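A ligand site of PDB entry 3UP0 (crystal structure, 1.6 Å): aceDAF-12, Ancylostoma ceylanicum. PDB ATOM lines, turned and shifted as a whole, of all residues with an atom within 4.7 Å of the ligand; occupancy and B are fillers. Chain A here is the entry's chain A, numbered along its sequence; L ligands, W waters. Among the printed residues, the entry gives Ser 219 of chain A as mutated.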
ATOM      1  N   MET A  27     -25.894   6.532   2.175  1.00  0.00           N
ATOM      2  CA  MET A  27     -25.686   7.950   1.903  1.00  0.00           C
ATOM      3  C   MET A  27     -25.954   8.282   0.437  1.00  0.00           C
ATOM      4  O   MET A  27     -25.482   7.562  -0.459  1.00  0.00           O
ATOM      5  CB  MET A  27     -24.243   8.367   2.228  1.00  0.00           C
ATOM      6  CG  MET A  27     -23.899   8.324   3.720  1.00  0.00           C
ATOM      7  SD  MET A  27     -22.166   8.763   4.030  1.00  0.00           S
ATOM      8  CE  MET A  27     -21.364   7.229   3.588  1.00  0.00           C
ATOM      9  N   PHE A  36     -16.313  10.303   2.662  1.00  0.00           N
ATOM     10  CA  PHE A  36     -16.204   8.991   3.297  1.00  0.00           C
ATOM     11  C   PHE A  36     -15.449   7.989   2.414  1.00  0.00           C
ATOM     12  O   PHE A  36     -14.684   7.188   2.906  1.00  0.00           O
ATOM     13  CB  PHE A  36     -17.588   8.425   3.635  1.00  0.00           C
ATOM     14  CG  PHE A  36     -17.529   7.227   4.551  1.00  0.00           C
ATOM     15  CD1 PHE A  36     -17.434   7.382   5.932  1.00  0.00           C
ATOM     16  CD2 PHE A  36     -17.566   5.933   4.027  1.00  0.00           C
ATOM     17  CE1 PHE A  36     -17.332   6.267   6.784  1.00  0.00           C
ATOM     18  CE2 PHE A  36     -17.492   4.795   4.871  1.00  0.00           C
ATOM     19  CZ  PHE A  36     -17.380   4.965   6.245  1.00  0.00           C
ATOM     20  N   ILE A  46     -13.277  14.667   7.465  1.00  0.00           N
ATOM     21  CA  ILE A  46     -13.816  14.114   8.721  1.00  0.00           C
ATOM     22  C   ILE A  46     -15.048  14.915   9.152  1.00  0.00           C
ATOM     23  O   ILE A  46     -16.046  14.343   9.597  1.00  0.00           O
ATOM     24  CB  ILE A  46     -12.773  14.100   9.826  1.00  0.00           C
ATOM     25  CG1 ILE A  46     -11.542  13.322   9.398  1.00  0.00           C
ATOM     26  CG2 ILE A  46     -13.373  13.537  11.118  1.00  0.00           C
ATOM     27  CD1 ILE A  46     -11.803  11.870   9.052  1.00  0.00           C
ATOM     28  N   ILE A  49     -18.036  13.933   7.082  1.00  0.00           N
ATOM     29  CA  ILE A  49     -18.540  12.643   7.532  1.00  0.00           C
ATOM     30  C   ILE A  49     -19.365  12.743   8.797  1.00  0.00           C
ATOM     31  O   ILE A  49     -20.490  12.192   8.849  1.00  0.00           O
ATOM     32  CB  ILE A  49     -17.343  11.644   7.749  1.00  0.00           C
ATOM     33  CG1 ILE A  49     -16.720  11.343   6.390  1.00  0.00           C
ATOM     34  CG2 ILE A  49     -17.827  10.360   8.409  1.00  0.00           C
ATOM     35  CD1 ILE A  49     -15.383  10.622   6.486  1.00  0.00           C
ATOM     36  N   MET A  50     -18.853  13.503   9.759  1.00  0.00           N
ATOM     37  CA  MET A  50     -19.603  13.747  11.011  1.00  0.00           C
ATOM     38  C   MET A  50     -20.962  14.373  10.740  1.00  0.00           C
ATOM     39  O   MET A  50     -21.933  14.038  11.452  1.00  0.00           O
ATOM     40  CB  MET A  50     -18.824  14.671  11.948  1.00  0.00           C
ATOM     41  CG  MET A  50     -17.636  13.987  12.547  1.00  0.00           C
ATOM     42  SD  MET A  50     -16.976  14.983  13.918  1.00  0.00           S
ATOM     43  CE  MET A  50     -16.263  16.370  13.079  1.00  0.00           C
ATOM     44  N   VAL A  52     -23.115  13.780   8.430  1.00  0.00           N
ATOM     45  CA  VAL A  52     -24.113  12.778   8.135  1.00  0.00           C
ATOM     46  C   VAL A  52     -24.724  12.223   9.430  1.00  0.00           C
ATOM     47  O   VAL A  52     -25.927  12.250   9.616  1.00  0.00           O
ATOM     48  CB  VAL A  52     -23.529  11.608   7.333  1.00  0.00           C
ATOM     49  CG1 VAL A  52     -24.568  10.547   7.073  1.00  0.00           C
ATOM     50  CG2 VAL A  52     -22.890  12.156   6.089  1.00  0.00           C
ATOM     51  N   THR A  53     -23.866  11.790  10.362  1.00  0.00           N
ATOM     52  CA  THR A  53     -24.325  11.229  11.608  1.00  0.00           C
ATOM     53  C   THR A  53     -25.068  12.248  12.459  1.00  0.00           C
ATOM     54  O   THR A  53     -26.086  11.941  13.066  1.00  0.00           O
ATOM     55  CB  THR A  53     -23.127  10.653  12.434  1.00  0.00           C
ATOM     56  OG1 THR A  53     -22.265   9.904  11.563  1.00  0.00           O
ATOM     57  CG2 THR A  53     -23.583   9.771  13.535  1.00  0.00           C
ATOM     58  N   LEU A  87     -22.217  11.083  19.228  1.00  0.00           N
ATOM     59  CA  LEU A  87     -21.304  10.738  18.106  1.00  0.00           C
ATOM     60  C   LEU A  87     -20.251   9.746  18.582  1.00  0.00           C
ATOM     61  O   LEU A  87     -19.854   8.836  17.873  1.00  0.00           O
ATOM     62  CB  LEU A  87     -20.620  11.954  17.532  1.00  0.00           C
ATOM     63  CG  LEU A  87     -21.255  12.820  16.494  1.00  0.00           C
ATOM     64  CD1 LEU A  87     -20.337  13.992  16.184  1.00  0.00           C
ATOM     65  CD2 LEU A  87     -21.481  11.945  15.261  1.00  0.00           C
ATOM     66  N   THR A  88     -19.752   9.963  19.806  1.00  0.00           N
ATOM     67  CA  THR A  88     -18.726   9.098  20.365  1.00  0.00           C
ATOM     68  C   THR A  88     -19.257   7.681  20.580  1.00  0.00           C
ATOM     69  O   THR A  88     -18.536   6.698  20.330  1.00  0.00           O
ATOM     70  CB  THR A  88     -18.117   9.697  21.659  1.00  0.00           C
ATOM     71  OG1 THR A  88     -17.619  11.007  21.351  1.00  0.00           O
ATOM     72  CG2 THR A  88     -16.958   8.833  22.177  1.00  0.00           C
ATOM     73  N   ARG A  90     -21.717   6.357  18.831  1.00  0.00           N
ATOM     74  CA  ARG A  90     -21.781   5.807  17.462  1.00  0.00           C
ATOM     75  C   ARG A  90     -20.408   5.321  17.065  1.00  0.00           C
ATOM     76  O   ARG A  90     -20.252   4.278  16.451  1.00  0.00           O
ATOM     77  CB  ARG A  90     -22.310   6.859  16.474  1.00  0.00           C
ATOM     78  CG  ARG A  90     -22.330   6.396  15.012  1.00  0.00           C
ATOM     79  CD  ARG A  90     -23.472   5.484  14.741  1.00  0.00           C
ATOM     80  NE  ARG A  90     -23.640   5.240  13.300  1.00  0.00           N
ATOM     81  CZ  ARG A  90     -24.495   4.357  12.797  1.00  0.00           C
ATOM     82  NH1 ARG A  90     -25.303   3.661  13.584  1.00  0.00           N
ATOM     83  NH2 ARG A  90     -24.558   4.181  11.487  1.00  0.00           N
ATOM     84  N   GLY A  91     -19.373   6.066  17.452  1.00  0.00           N
ATOM     85  CA  GLY A  91     -18.003   5.684  17.214  1.00  0.00           C
ATOM     86  C   GLY A  91     -17.638   4.336  17.796  1.00  0.00           C
ATOM     87  O   GLY A  91     -16.939   3.549  17.169  1.00  0.00           O
ATOM     88  N   ARG A  94     -19.209   1.536  15.727  1.00  0.00           N
ATOM     89  CA  ARG A  94     -18.656   1.391  14.382  1.00  0.00           C
ATOM     90  C   ARG A  94     -17.156   1.120  14.313  1.00  0.00           C
ATOM     91  O   ARG A  94     -16.590   0.998  13.202  1.00  0.00           O
ATOM     92  CB  ARG A  94     -19.011   2.621  13.548  1.00  0.00           C
ATOM     93  CG  ARG A  94     -20.510   2.854  13.315  1.00  0.00           C
ATOM     94  CD  ARG A  94     -21.300   1.597  12.923  1.00  0.00           C
ATOM     95  NE  ARG A  94     -20.615   0.927  11.835  1.00  0.00           N
ATOM     96  CZ  ARG A  94     -20.910  -0.317  11.410  1.00  0.00           C
ATOM     97  NH1 ARG A  94     -21.872  -1.014  11.982  1.00  0.00           N
ATOM     98  NH2 ARG A  94     -20.196  -0.855  10.429  1.00  0.00           N
ATOM     99  N   TRP A 102     -13.052   3.039  11.688  1.00  0.00           N
ATOM    100  CA  TRP A 102     -14.479   3.057  11.713  1.00  0.00           C
ATOM    101  C   TRP A 102     -15.036   2.722  10.315  1.00  0.00           C
ATOM    102  O   TRP A 102     -14.459   3.164   9.336  1.00  0.00           O
ATOM    103  CB  TRP A 102     -15.003   4.429  12.064  1.00  0.00           C
ATOM    104  CG  TRP A 102     -14.697   4.888  13.502  1.00  0.00           C
ATOM    105  CD1 TRP A 102     -15.371   4.547  14.600  1.00  0.00           C
ATOM    106  CD2 TRP A 102     -13.703   5.831  13.900  1.00  0.00           C
ATOM    107  NE1 TRP A 102     -14.859   5.209  15.711  1.00  0.00           N
ATOM    108  CE2 TRP A 102     -13.825   5.991  15.296  1.00  0.00           C
ATOM    109  CE3 TRP A 102     -12.722   6.546  13.224  1.00  0.00           C
ATOM    110  CZ2 TRP A 102     -13.004   6.869  16.001  1.00  0.00           C
ATOM    111  CZ3 TRP A 102     -11.902   7.435  13.963  1.00  0.00           C
ATOM    112  CH2 TRP A 102     -12.056   7.550  15.327  1.00  0.00           C
ATOM    113  N   THR A 103     -16.136   1.995  10.274  1.00  0.00           N
ATOM    114  CA  THR A 103     -16.862   1.723   9.026  1.00  0.00           C
ATOM    115  C   THR A 103     -18.339   2.129   9.178  1.00  0.00           C
ATOM    116  O   THR A 103     -18.797   2.429  10.274  1.00  0.00           O
ATOM    117  CB  THR A 103     -16.781   0.237   8.675  1.00  0.00           C
ATOM    118  OG1 THR A 103     -17.289  -0.531   9.775  1.00  0.00           O
ATOM    119  CG2 THR A 103     -15.339  -0.159   8.381  1.00  0.00           C
ATOM    120  N   THR A 104     -19.071   2.151   8.065  1.00  0.00           N
ATOM    121  CA  THR A 104     -20.494   2.454   8.075  1.00  0.00           C
ATOM    122  C   THR A 104     -21.249   1.193   7.594  1.00  0.00           C
ATOM    123  O   THR A 104     -20.714   0.443   6.777  1.00  0.00           O
ATOM    124  CB  THR A 104     -20.798   3.669   7.174  1.00  0.00           C
ATOM    125  OG1 THR A 104     -22.098   4.155   7.452  1.00  0.00           O
ATOM    126  CG2 THR A 104     -20.724   3.291   5.665  1.00  0.00           C
ATOM    127  N   PRO A 105     -22.452   0.925   8.148  1.00  0.00           N
ATOM    128  CA  PRO A 105     -23.157  -0.364   7.943  1.00  0.00           C
ATOM    129  C   PRO A 105     -23.563  -0.708   6.524  1.00  0.00           C
ATOM    130  O   PRO A 105     -23.678  -1.898   6.211  1.00  0.00           O
ATOM    131  CB  PRO A 105     -24.402  -0.215   8.817  1.00  0.00           C
ATOM    132  CG  PRO A 105     -24.477   1.207   9.132  1.00  0.00           C
ATOM    133  CD  PRO A 105     -23.108   1.679   9.221  1.00  0.00           C
ATOM    134  N   VAL A 113     -12.770   5.106   8.022  1.00  0.00           N
ATOM    135  CA  VAL A 113     -12.018   6.211   8.540  1.00  0.00           C
ATOM    136  C   VAL A 113     -10.997   5.635   9.532  1.00  0.00           C
ATOM    137  O   VAL A 113     -11.395   4.974  10.495  1.00  0.00           O
ATOM    138  CB  VAL A 113     -12.958   7.173   9.293  1.00  0.00           C
ATOM    139  CG1 VAL A 113     -12.158   8.304   9.911  1.00  0.00           C
ATOM    140  CG2 VAL A 113     -14.015   7.730   8.351  1.00  0.00           C
ATOM    141  N   MET A 117      -6.745   9.360  11.751  1.00  0.00           N
ATOM    142  CA  MET A 117      -7.273  10.677  11.396  1.00  0.00           C
ATOM    143  C   MET A 117      -6.977  11.701  12.495  1.00  0.00           C
ATOM    144  O   MET A 117      -6.812  12.895  12.232  1.00  0.00           O
ATOM    145  CB  MET A 117      -8.773  10.603  11.066  1.00  0.00           C
ATOM    146  CG  MET A 117      -9.714  10.399  12.234  1.00  0.00           C
ATOM    147  SD  MET A 117     -10.185  11.939  12.991  1.00  0.00           S
ATOM    148  CE  MET A 117     -11.012  11.337  14.492  1.00  0.00           C
ATOM    149  N   PHE A 118      -6.894  11.214  13.748  1.00  0.00           N
ATOM    150  CA  PHE A 118      -6.610  12.092  14.858  1.00  0.00           C
ATOM    151  C   PHE A 118      -5.282  12.841  14.672  1.00  0.00           C
ATOM    152  O   PHE A 118      -5.131  13.988  15.091  1.00  0.00           O
ATOM    153  CB  PHE A 118      -6.540  11.325  16.183  1.00  0.00           C
ATOM    154  CG  PHE A 118      -7.867  11.124  16.881  1.00  0.00           C
ATOM    155  CD1 PHE A 118      -8.491  12.201  17.535  1.00  0.00           C
ATOM    156  CD2 PHE A 118      -8.463   9.878  16.939  1.00  0.00           C
ATOM    157  CE1 PHE A 118      -9.702  12.016  18.223  1.00  0.00           C
ATOM    158  CE2 PHE A 118      -9.632   9.705  17.617  1.00  0.00           C
ATOM    159  CZ  PHE A 118     -10.254  10.760  18.269  1.00  0.00           C
ATOM    160  N   GLN A 129      -6.909  13.173  22.781  1.00  0.00           N
ATOM    161  CA  GLN A 129      -8.264  12.744  22.389  1.00  0.00           C
ATOM    162  C   GLN A 129      -8.266  11.365  21.766  1.00  0.00           C
ATOM    163  O   GLN A 129      -9.192  10.598  21.962  1.00  0.00           O
ATOM    164  CB  GLN A 129      -8.909  13.779  21.478  1.00  0.00           C
ATOM    165  CG  GLN A 129      -9.187  15.104  22.140  1.00  0.00           C
ATOM    166  CD  GLN A 129      -9.795  14.992  23.507  1.00  0.00           C
ATOM    167  OE1 GLN A 129      -9.077  15.059  24.498  1.00  0.00           O
ATOM    168  NE2 GLN A 129     -11.115  14.819  23.577  1.00  0.00           N
ATOM    169  N   PHE A 133     -10.435   8.201  23.258  1.00  0.00           N
ATOM    170  CA  PHE A 133     -11.388   7.418  22.512  1.00  0.00           C
ATOM    171  C   PHE A 133     -11.052   5.900  22.619  1.00  0.00           C
ATOM    172  O   PHE A 133     -11.932   5.088  22.834  1.00  0.00           O
ATOM    173  CB  PHE A 133     -11.485   7.806  21.029  1.00  0.00           C
ATOM    174  CG  PHE A 133     -12.424   6.923  20.302  1.00  0.00           C
ATOM    175  CD1 PHE A 133     -13.784   7.101  20.406  1.00  0.00           C
ATOM    176  CD2 PHE A 133     -11.961   5.811  19.647  1.00  0.00           C
ATOM    177  CE1 PHE A 133     -14.666   6.192  19.815  1.00  0.00           C
ATOM    178  CE2 PHE A 133     -12.858   4.931  19.024  1.00  0.00           C
ATOM    179  CZ  PHE A 133     -14.193   5.119  19.130  1.00  0.00           C
ATOM    180  N   ILE A 215     -14.877  13.132  27.407  1.00  0.00           N
ATOM    181  CA  ILE A 215     -14.533  13.247  25.995  1.00  0.00           C
ATOM    182  C   ILE A 215     -15.192  14.489  25.410  1.00  0.00           C
ATOM    183  O   ILE A 215     -14.539  15.257  24.679  1.00  0.00           O
ATOM    184  CB  ILE A 215     -14.926  11.952  25.238  1.00  0.00           C
ATOM    185  CG1 ILE A 215     -13.929  10.870  25.562  1.00  0.00           C
ATOM    186  CG2 ILE A 215     -15.042  12.221  23.713  1.00  0.00           C
ATOM    187  CD1 ILE A 215     -14.335   9.457  25.150  1.00  0.00           C
ATOM    188  N   SER A 219     -13.066  17.850  23.676  1.00  0.00           N
ATOM    189  CA  SER A 219     -13.000  17.715  22.210  1.00  0.00           C
ATOM    190  C   SER A 219     -13.245  19.000  21.430  1.00  0.00           C
ATOM    191  O   SER A 219     -12.984  19.039  20.227  1.00  0.00           O
ATOM    192  CB  SER A 219     -13.978  16.636  21.716  1.00  0.00           C
ATOM    193  OG  SER A 219     -13.650  15.359  22.178  1.00  0.00           O
ATOM    194  N   LEU A 222     -10.609  20.390  18.858  1.00  0.00           N
ATOM    195  CA  LEU A 222      -9.886  19.422  18.086  1.00  0.00           C
ATOM    196  C   LEU A 222      -9.645  19.795  16.629  1.00  0.00           C
ATOM    197  O   LEU A 222      -8.652  19.358  16.041  1.00  0.00           O
ATOM    198  CB  LEU A 222     -10.616  18.087  18.154  1.00  0.00           C
ATOM    199  CG  LEU A 222      -9.970  16.808  17.679  1.00  0.00           C
ATOM    200  CD1 LEU A 222      -8.640  16.556  18.364  1.00  0.00           C
ATOM    201  CD2 LEU A 222     -10.965  15.671  18.009  1.00  0.00           C
ATOM    202  N   PHE A 223     -10.546  20.578  16.055  1.00  0.00           N
ATOM    203  CA  PHE A 223     -10.414  20.947  14.636  1.00  0.00           C
ATOM    204  C   PHE A 223      -9.872  22.366  14.452  1.00  0.00           C
ATOM    205  O   PHE A 223      -9.752  22.828  13.312  1.00  0.00           O
ATOM    206  CB  PHE A 223     -11.727  20.777  13.893  1.00  0.00           C
ATOM    207  CG  PHE A 223     -12.132  19.328  13.756  1.00  0.00           C
ATOM    208  CD1 PHE A 223     -12.804  18.682  14.794  1.00  0.00           C
ATOM    209  CD2 PHE A 223     -11.849  18.592  12.597  1.00  0.00           C
ATOM    210  CE1 PHE A 223     -13.128  17.329  14.694  1.00  0.00           C
ATOM    211  CE2 PHE A 223     -12.209  17.250  12.502  1.00  0.00           C
ATOM    212  CZ  PHE A 223     -12.844  16.628  13.542  1.00  0.00           C
HETATM  213  O1  LIG L   1     -22.638   5.330   9.743  1.00  0.00           O
HETATM  214  C1  LIG L   1     -22.249   6.493  10.013  1.00  0.00           C
HETATM  215  O2  LIG L   1     -22.704   7.089  11.060  1.00  0.00           O
HETATM  216  C2  LIG L   1     -21.225   7.174   9.109  1.00  0.00           C
HETATM  217  C3  LIG L   1     -21.881   8.392   8.441  1.00  0.00           C
HETATM  218  C4  LIG L   1     -19.993   7.649   9.859  1.00  0.00           C
HETATM  219  C5  LIG L   1     -19.251   6.475  10.496  1.00  0.00           C
HETATM  220  C6  LIG L   1     -17.938   6.920  11.166  1.00  0.00           C
HETATM  221  C7  LIG L   1     -18.130   7.812  12.401  1.00  0.00           C
HETATM  222  C8  LIG L   1     -18.973   7.091  13.468  1.00  0.00           C
HETATM  223  C9  LIG L   1     -16.782   8.313  12.961  1.00  0.00           C
HETATM  224  C10 LIG L   1     -15.978   9.128  11.922  1.00  0.00           C
HETATM  225  C11 LIG L   1     -15.177  10.211  12.633  1.00  0.00           C
HETATM  226  C12 LIG L   1     -15.346   9.845  14.103  1.00  0.00           C
HETATM  227  C13 LIG L   1     -15.061  10.908  15.161  1.00  0.00           C
HETATM  228  C14 LIG L   1     -14.558  12.134  14.897  1.00  0.00           C
HETATM  229  C15 LIG L   1     -14.172  13.082  16.004  1.00  0.00           C
HETATM  230  C16 LIG L   1     -16.738   9.245  14.196  1.00  0.00           C
HETATM  231  C17 LIG L   1     -17.841  10.319  14.112  1.00  0.00           C
HETATM  232  C18 LIG L   1     -16.814   8.569  15.559  1.00  0.00           C
HETATM  233  C19 LIG L   1     -16.566   9.569  16.706  1.00  0.00           C
HETATM  234  C20 LIG L   1     -15.268  10.406  16.627  1.00  0.00           C
HETATM  235  C21 LIG L   1     -15.089  11.477  17.729  1.00  0.00           C
HETATM  236  C22 LIG L   1     -14.706  10.767  19.057  1.00  0.00           C
HETATM  237  C23 LIG L   1     -16.347  12.317  17.886  1.00  0.00           C
HETATM  238  C24 LIG L   1     -13.934  12.406  17.362  1.00  0.00           C
HETATM  239  C25 LIG L   1     -13.512  13.384  18.453  1.00  0.00           C
HETATM  240  C26 LIG L   1     -13.298  12.678  19.777  1.00  0.00           C
HETATM  241  O3  LIG L   1     -12.315  12.910  20.462  1.00  0.00           O
HETATM  242  C27 LIG L   1     -14.381  11.726  20.200  1.00  0.00           C
HETATM  243  O   HOH W   1     -25.468   7.466  10.573  1.00  0.00           O
HETATM  244  O   HOH W   2     -11.852  11.075  22.529  1.00  0.00           O
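Residues that only touch the ligand: Leu 222 (3.5 Å), Thr 88 (3.5 Å), Gly 91 (3.5 Å), Phe 118 (3.6 Å), Leu 87 (3.6 Å), Ile 215 (3.6 Å), Met 117 (3.7 Å), Gln 129 (3.7 Å), Val 52 (3.7 Å), Pro 105 (3.7 Å), Ile 49 (3.8 Å), Met 50 (3.9 Å) and Trp 102 (3.9 Å). Hydrophobic or aromatic side chains within 4 Å of the ligand: Ile 49, Met 50, Val 52, Trp 102, Pro 105, Met 117, Phe 118, Ile 215 and Leu 222. Of the 25 residues printed, 17 come within 4 Å of the ligand. The nearest printed residue that does not touch the ligand is Phe 133 (4.01 Å).
Water W2 lies within hydrogen-bond range of O of Gln 129 (2.8 Å), O3 of the ligand (2.8 Å) and N of Phe 133 (3.3 Å).
O of Ile 215 is in hydrogen-bond range of OG of Ser 219, 2.7 Å away. The side-chain hydroxyl (OG) of Ser 219 is in hydrogen-bond range of the side-chain amide nitrogen (NE2) of Gln 129 (2.9 Å). The backbone carbonyl oxygen (O) of Gly 91 is in hydrogen-bond range of the indole nitrogen (NE1) of Trp 102 (3.0 Å). N of Trp 102 lies within hydrogen-bond range of O of Val 113 (2.8 Å).
An oxygen (O1) of the ligand is in hydrogen-bond range of the side-chain hydroxyl (OG1) of Thr 104, at 2.6 Å. The guanidinium group of Arg 90 lies within salt-bridge range of an oxygen (O1) of the ligand, at 2.8 Å. An oxygen (O2) of the ligand lies within hydrogen-bond range of the side-chain hydroxyl of Thr 53, 2.9 Å away. OG of Ser 219 sits at hydrogen-bond distance from O3 of the ligand, at 3.3 Å.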
